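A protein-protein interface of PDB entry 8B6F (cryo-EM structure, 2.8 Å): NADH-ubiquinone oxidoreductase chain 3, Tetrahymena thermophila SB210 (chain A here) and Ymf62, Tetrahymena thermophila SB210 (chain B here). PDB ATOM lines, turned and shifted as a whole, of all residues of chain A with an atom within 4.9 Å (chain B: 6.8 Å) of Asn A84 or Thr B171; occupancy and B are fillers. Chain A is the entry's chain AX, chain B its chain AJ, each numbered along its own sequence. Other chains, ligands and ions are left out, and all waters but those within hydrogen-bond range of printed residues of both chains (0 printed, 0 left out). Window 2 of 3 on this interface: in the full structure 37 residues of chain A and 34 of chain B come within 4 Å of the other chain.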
ATOM      1  N   PRO A  80      22.419  17.260 -15.227  1.00  0.00           N
ATOM      2  CA  PRO A  80      21.168  17.265 -14.446  1.00  0.00           C
ATOM      3  C   PRO A  80      20.251  16.091 -14.745  1.00  0.00           C
ATOM      4  O   PRO A  80      19.637  15.544 -13.821  1.00  0.00           O
ATOM      5  CB  PRO A  80      20.524  18.610 -14.820  1.00  0.00           C
ATOM      6  CG  PRO A  80      21.173  19.022 -16.082  1.00  0.00           C
ATOM      7  CD  PRO A  80      22.565  18.485 -16.033  1.00  0.00           C
ATOM      8  N   VAL A  81      20.131  15.685 -16.010  1.00  0.00           N
ATOM      9  CA  VAL A  81      19.244  14.573 -16.338  1.00  0.00           C
ATOM     10  C   VAL A  81      19.797  13.265 -15.783  1.00  0.00           C
ATOM     11  O   VAL A  81      19.041  12.408 -15.313  1.00  0.00           O
ATOM     12  CB  VAL A  81      19.010  14.495 -17.859  1.00  0.00           C
ATOM     13  CG1 VAL A  81      20.323  14.377 -18.617  1.00  0.00           C
ATOM     14  CG2 VAL A  81      18.090  13.333 -18.203  1.00  0.00           C
ATOM     15  N   LEU A  82      21.119  13.089 -15.825  1.00  0.00           N
ATOM     16  CA  LEU A  82      21.723  11.898 -15.236  1.00  0.00           C
ATOM     17  C   LEU A  82      21.516  11.868 -13.728  1.00  0.00           C
ATOM     18  O   LEU A  82      21.222  10.813 -13.155  1.00  0.00           O
ATOM     19  CB  LEU A  82      23.211  11.847 -15.572  1.00  0.00           C
ATOM     20  CG  LEU A  82      23.545  11.782 -17.064  1.00  0.00           C
ATOM     21  CD1 LEU A  82      25.026  12.011 -17.281  1.00  0.00           C
ATOM     22  CD2 LEU A  82      23.114  10.455 -17.663  1.00  0.00           C
ATOM     23  N   PHE A  83      21.666  13.017 -13.068  1.00  0.00           N
ATOM     24  CA  PHE A  83      21.489  13.069 -11.622  1.00  0.00           C
ATOM     25  C   PHE A  83      20.053  12.756 -11.226  1.00  0.00           C
ATOM     26  O   PHE A  83      19.814  12.035 -10.251  1.00  0.00           O
ATOM     27  CB  PHE A  83      21.903  14.442 -11.093  1.00  0.00           C
ATOM     28  CG  PHE A  83      23.356  14.537 -10.737  1.00  0.00           C
ATOM     29  CD1 PHE A  83      24.326  14.596 -11.721  1.00  0.00           C
ATOM     30  CD2 PHE A  83      23.751  14.577  -9.412  1.00  0.00           C
ATOM     31  CE1 PHE A  83      25.663  14.687 -11.390  1.00  0.00           C
ATOM     32  CE2 PHE A  83      25.085  14.668  -9.076  1.00  0.00           C
ATOM     33  CZ  PHE A  83      26.043  14.724 -10.065  1.00  0.00           C
ATOM     34  N   ASN A  84      19.084  13.288 -11.965  1.00  0.00           N
ATOM     35  CA  ASN A  84      17.669  13.132 -11.647  1.00  0.00           C
ATOM     36  C   ASN A  84      16.962  12.233 -12.656  1.00  0.00           C
ATOM     37  O   ASN A  84      15.810  12.470 -13.022  1.00  0.00           O
ATOM     38  CB  ASN A  84      16.983  14.493 -11.587  1.00  0.00           C
ATOM     39  CG  ASN A  84      17.563  15.389 -10.515  1.00  0.00           C
ATOM     40  OD1 ASN A  84      17.288  15.214  -9.329  1.00  0.00           O
ATOM     41  ND2 ASN A  84      18.361  16.364 -10.928  1.00  0.00           N
ATOM     42  N   PHE A  85      17.646  11.188 -13.124  1.00  0.00           N
ATOM     43  CA  PHE A  85      17.023  10.266 -14.064  1.00  0.00           C
ATOM     44  C   PHE A  85      15.916   9.442 -13.421  1.00  0.00           C
ATOM     45  O   PHE A  85      15.102   8.858 -14.141  1.00  0.00           O
ATOM     46  CB  PHE A  85      18.068   9.337 -14.676  1.00  0.00           C
ATOM     47  CG  PHE A  85      17.577   8.603 -15.889  1.00  0.00           C
ATOM     48  CD1 PHE A  85      17.598   9.204 -17.136  1.00  0.00           C
ATOM     49  CD2 PHE A  85      17.101   7.307 -15.784  1.00  0.00           C
ATOM     50  CE1 PHE A  85      17.143   8.530 -18.252  1.00  0.00           C
ATOM     51  CE2 PHE A  85      16.648   6.628 -16.895  1.00  0.00           C
ATOM     52  CZ  PHE A  85      16.671   7.239 -18.132  1.00  0.00           C
ATOM     53  N   SER A  86      15.867   9.375 -12.089  1.00  0.00           N
ATOM     54  CA  SER A  86      14.738   8.736 -11.427  1.00  0.00           C
ATOM     55  C   SER A  86      13.446   9.514 -11.634  1.00  0.00           C
ATOM     56  O   SER A  86      12.362   8.939 -11.497  1.00  0.00           O
ATOM     57  CB  SER A  86      15.017   8.581  -9.932  1.00  0.00           C
ATOM     58  OG  SER A  86      15.172   9.842  -9.305  1.00  0.00           O
ATOM     59  N   MET A  87      13.540  10.801 -11.958  1.00  0.00           N
ATOM     60  CA  MET A  87      12.383  11.641 -12.235  1.00  0.00           C
ATOM     61  C   MET A  87      12.039  11.693 -13.716  1.00  0.00           C
ATOM     62  O   MET A  87      11.175  12.483 -14.110  1.00  0.00           O
ATOM     63  CB  MET A  87      12.631  13.065 -11.727  1.00  0.00           C
ATOM     64  CG  MET A  87      13.073  13.154 -10.273  1.00  0.00           C
ATOM     65  SD  MET A  87      13.453  14.849  -9.784  1.00  0.00           S
ATOM     66  CE  MET A  87      14.039  14.599  -8.113  1.00  0.00           C
ATOM     67  N   PHE A  88      12.694  10.883 -14.543  1.00  0.00           N
ATOM     68  CA  PHE A  88      12.535  11.005 -15.985  1.00  0.00           C
ATOM     69  C   PHE A  88      11.088  10.763 -16.392  1.00  0.00           C
ATOM     70  O   PHE A  88      10.384   9.942 -15.799  1.00  0.00           O
ATOM     71  CB  PHE A  88      13.452  10.017 -16.705  1.00  0.00           C
ATOM     72  CG  PHE A  88      12.855   8.648 -16.874  1.00  0.00           C
ATOM     73  CD1 PHE A  88      12.909   7.722 -15.848  1.00  0.00           C
ATOM     74  CD2 PHE A  88      12.254   8.285 -18.068  1.00  0.00           C
ATOM     75  CE1 PHE A  88      12.364   6.462 -16.002  1.00  0.00           C
ATOM     76  CE2 PHE A  88      11.708   7.027 -18.230  1.00  0.00           C
ATOM     77  CZ  PHE A  88      11.763   6.115 -17.195  1.00  0.00           C
ATOM     78  N   GLU A  92      11.478  14.260 -20.918  1.00  0.00           N
ATOM     79  CA  GLU A  92      12.881  14.290 -20.520  1.00  0.00           C
ATOM     80  C   GLU A  92      13.672  13.193 -21.217  1.00  0.00           C
ATOM     81  O   GLU A  92      14.796  13.422 -21.677  1.00  0.00           O
ATOM     82  CB  GLU A  92      12.998  14.158 -19.003  1.00  0.00           C
ATOM     83  CG  GLU A  92      12.222  15.218 -18.244  1.00  0.00           C
ATOM     84  CD  GLU A  92      12.422  15.122 -16.747  1.00  0.00           C
ATOM     85  OE1 GLU A  92      13.314  14.363 -16.316  1.00  0.00           O
ATOM     86  OE2 GLU A  92      11.684  15.800 -16.002  1.00  0.00           O
ATOM     87  N   ILE B 166      14.158  15.326  -2.716  1.00  0.00           N
ATOM     88  CA  ILE B 166      15.313  15.681  -3.527  1.00  0.00           C
ATOM     89  C   ILE B 166      16.593  15.496  -2.721  1.00  0.00           C
ATOM     90  O   ILE B 166      16.626  15.703  -1.501  1.00  0.00           O
ATOM     91  CB  ILE B 166      15.176  17.128  -4.038  1.00  0.00           C
ATOM     92  CG1 ILE B 166      13.941  17.254  -4.934  1.00  0.00           C
ATOM     93  CG2 ILE B 166      16.425  17.557  -4.798  1.00  0.00           C
ATOM     94  CD1 ILE B 166      13.518  18.681  -5.189  1.00  0.00           C
ATOM     95  N   MET B 167      17.665  15.108  -3.416  1.00  0.00           N
ATOM     96  CA  MET B 167      18.959  14.889  -2.788  1.00  0.00           C
ATOM     97  C   MET B 167      20.116  15.562  -3.513  1.00  0.00           C
ATOM     98  O   MET B 167      21.251  15.483  -3.032  1.00  0.00           O
ATOM     99  CB  MET B 167      19.250  13.385  -2.680  1.00  0.00           C
ATOM    100  CG  MET B 167      18.596  12.725  -1.485  1.00  0.00           C
ATOM    101  SD  MET B 167      19.307  13.269   0.081  1.00  0.00           S
ATOM    102  CE  MET B 167      20.908  12.471   0.025  1.00  0.00           C
ATOM    103  N   ASN B 168      19.872  16.210  -4.650  1.00  0.00           N
ATOM    104  CA  ASN B 168      20.908  16.914  -5.388  1.00  0.00           C
ATOM    105  C   ASN B 168      20.432  18.325  -5.701  1.00  0.00           C
ATOM    106  O   ASN B 168      19.239  18.631  -5.635  1.00  0.00           O
ATOM    107  CB  ASN B 168      21.285  16.181  -6.684  1.00  0.00           C
ATOM    108  CG  ASN B 168      20.107  16.005  -7.619  1.00  0.00           C
ATOM    109  OD1 ASN B 168      19.792  16.889  -8.413  1.00  0.00           O
ATOM    110  ND2 ASN B 168      19.454  14.853  -7.535  1.00  0.00           N
ATOM    111  N   ASP B 169      21.389  19.188  -6.038  1.00  0.00           N
ATOM    112  CA  ASP B 169      21.115  20.584  -6.347  1.00  0.00           C
ATOM    113  C   ASP B 169      20.953  20.829  -7.841  1.00  0.00           C
ATOM    114  O   ASP B 169      21.099  21.969  -8.294  1.00  0.00           O
ATOM    115  CB  ASP B 169      22.226  21.473  -5.788  1.00  0.00           C
ATOM    116  CG  ASP B 169      22.318  21.407  -4.279  1.00  0.00           C
ATOM    117  OD1 ASP B 169      21.268  21.243  -3.626  1.00  0.00           O
ATOM    118  OD2 ASP B 169      23.441  21.519  -3.746  1.00  0.00           O
ATOM    119  N   PHE B 170      20.662  19.788  -8.615  1.00  0.00           N
ATOM    120  CA  PHE B 170      20.422  19.913 -10.046  1.00  0.00           C
ATOM    121  C   PHE B 170      18.940  19.990 -10.385  1.00  0.00           C
ATOM    122  O   PHE B 170      18.589  20.005 -11.568  1.00  0.00           O
ATOM    123  CB  PHE B 170      21.058  18.742 -10.796  1.00  0.00           C
ATOM    124  CG  PHE B 170      22.556  18.788 -10.838  1.00  0.00           C
ATOM    125  CD1 PHE B 170      23.310  18.199  -9.837  1.00  0.00           C
ATOM    126  CD2 PHE B 170      23.211  19.408 -11.889  1.00  0.00           C
ATOM    127  CE1 PHE B 170      24.689  18.238  -9.878  1.00  0.00           C
ATOM    128  CE2 PHE B 170      24.589  19.450 -11.935  1.00  0.00           C
ATOM    129  CZ  PHE B 170      25.330  18.863 -10.930  1.00  0.00           C
ATOM    130  N   THR B 171      18.065  20.044  -9.382  1.00  0.00           N
ATOM    131  CA  THR B 171      16.630  20.034  -9.658  1.00  0.00           C
ATOM    132  C   THR B 171      16.189  21.242 -10.470  1.00  0.00           C
ATOM    133  O   THR B 171      15.462  21.060 -11.461  1.00  0.00           O
ATOM    134  CB  THR B 171      15.850  19.921  -8.345  1.00  0.00           C
ATOM    135  OG1 THR B 171      16.097  18.641  -7.752  1.00  0.00           O
ATOM    136  CG2 THR B 171      14.351  20.075  -8.586  1.00  0.00           C
ATOM    137  N   PRO B 172      16.554  22.478 -10.121  1.00  0.00           N
ATOM    138  CA  PRO B 172      16.193  23.596 -11.008  1.00  0.00           C
ATOM    139  C   PRO B 172      16.777  23.456 -12.399  1.00  0.00           C
ATOM    140  O   PRO B 172      16.123  23.814 -13.385  1.00  0.00           O
ATOM    141  CB  PRO B 172      16.755  24.822 -10.273  1.00  0.00           C
ATOM    142  CG  PRO B 172      16.914  24.390  -8.866  1.00  0.00           C
ATOM    143  CD  PRO B 172      17.277  22.944  -8.927  1.00  0.00           C
ATOM    144  N   LEU B 173      18.004  22.946 -12.507  1.00  0.00           N
ATOM    145  CA  LEU B 173      18.633  22.812 -13.815  1.00  0.00           C
ATOM    146  C   LEU B 173      17.875  21.827 -14.696  1.00  0.00           C
ATOM    147  O   LEU B 173      17.676  22.079 -15.890  1.00  0.00           O
ATOM    148  CB  LEU B 173      20.090  22.384 -13.643  1.00  0.00           C
ATOM    149  CG  LEU B 173      20.983  23.398 -12.920  1.00  0.00           C
ATOM    150  CD1 LEU B 173      22.369  22.826 -12.690  1.00  0.00           C
ATOM    151  CD2 LEU B 173      21.073  24.707 -13.691  1.00  0.00           C
ATOM    152  N   THR B 174      17.448  20.694 -14.132  1.00  0.00           N
ATOM    153  CA  THR B 174      16.682  19.730 -14.918  1.00  0.00           C
ATOM    154  C   THR B 174      15.290  20.258 -15.239  1.00  0.00           C
ATOM    155  O   THR B 174      14.796  20.078 -16.358  1.00  0.00           O
ATOM    156  CB  THR B 174      16.599  18.384 -14.192  1.00  0.00           C
ATOM    157  OG1 THR B 174      15.842  17.459 -14.983  1.00  0.00           O
ATOM    158  CG2 THR B 174      15.943  18.525 -12.838  1.00  0.00           C
ATOM    159  N   LEU B 175      14.637  20.905 -14.272  1.00  0.00           N
ATOM    160  CA  LEU B 175      13.323  21.482 -14.534  1.00  0.00           C
ATOM    161  C   LEU B 175      13.381  22.554 -15.607  1.00  0.00           C
ATOM    162  O   LEU B 175      12.374  22.827 -16.268  1.00  0.00           O
ATOM    163  CB  LEU B 175      12.745  22.068 -13.247  1.00  0.00           C
ATOM    164  CG  LEU B 175      12.044  21.083 -12.319  1.00  0.00           C
ATOM    165  CD1 LEU B 175      11.832  21.692 -10.950  1.00  0.00           C
ATOM    166  CD2 LEU B 175      10.716  20.688 -12.937  1.00  0.00           C
ATOM    167  N   SER B 176      14.537  23.185 -15.786  1.00  0.00           N
ATOM    168  CA  SER B 176      14.693  24.191 -16.824  1.00  0.00           C
ATOM    169  C   SER B 176      15.074  23.599 -18.176  1.00  0.00           C
ATOM    170  O   SER B 176      14.413  23.866 -19.183  1.00  0.00           O
ATOM    171  CB  SER B 176      15.745  25.208 -16.410  1.00  0.00           C
ATOM    172  OG  SER B 176      15.811  26.206 -17.398  1.00  0.00           O
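The side-chain amide oxygen (OD1) of Asn A84 sits at hydrogen-bond distance from the side-chain amide nitrogen (ND2) of Asn B168 (2.8 Å).
O of Pro A80 is in hydrogen-bond range of ND2 of Asn A84, at 3.3 Å. The side-chain amide oxygen (OD1) of Asn B168 is in hydrogen-bond range of the backbone NH (N) of Phe B170 (3.0 Å).
Among the printed residues, merely in contact across the chains: Pro A80 with Phe B170 (3.9 Å), Pro A80 with Leu B173 (3.98 Å), Pro A80 with Thr B174 (3.8 Å), Phe A83 with Asn B168 (3.9 Å), Phe A83 with Phe B170 (3.7 Å), Asn A84 with Phe B170 (3.6 Å), Asn A84 with Thr B171 (3.96 Å) and Asn A84 with Thr B174 (3.8 Å).
Asn A84 touches just these residues of chain B: Asn B168, Phe B170, Thr B171 and Thr B174. Of chain A, only Asn A84 comes within 4 Å of Thr B171. Of the printed residues of chain A, Phe B170 touches Pro A80 (3.9 Å), Phe A83 (3.7 Å) and Asn A84 (3.6 Å). Of the printed residues of chain A, Thr B174 touches Pro A80 and Asn A84. Of the printed residues of chain A, Asn B168 touches Phe A83 (3.9 Å) and Asn A84 (2.8 Å). The nearest residue of chain A that does not touch Thr B171 is Met A87 (4.6 Å). The nearest printed residue of chain A that does not touch Asn B168 is Met A87 (5.5 Å).
Hydrophobic or aromatic side chains of chain B that line the printed part of chain A: Phe B170 and Leu B173. Among the printed residues, 9 pairs touch across the chains. Among the printed residues, no Asp or Glu carboxylate lies within 4 Å of a Lys or Arg side-chain nitrogen of the other chain.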
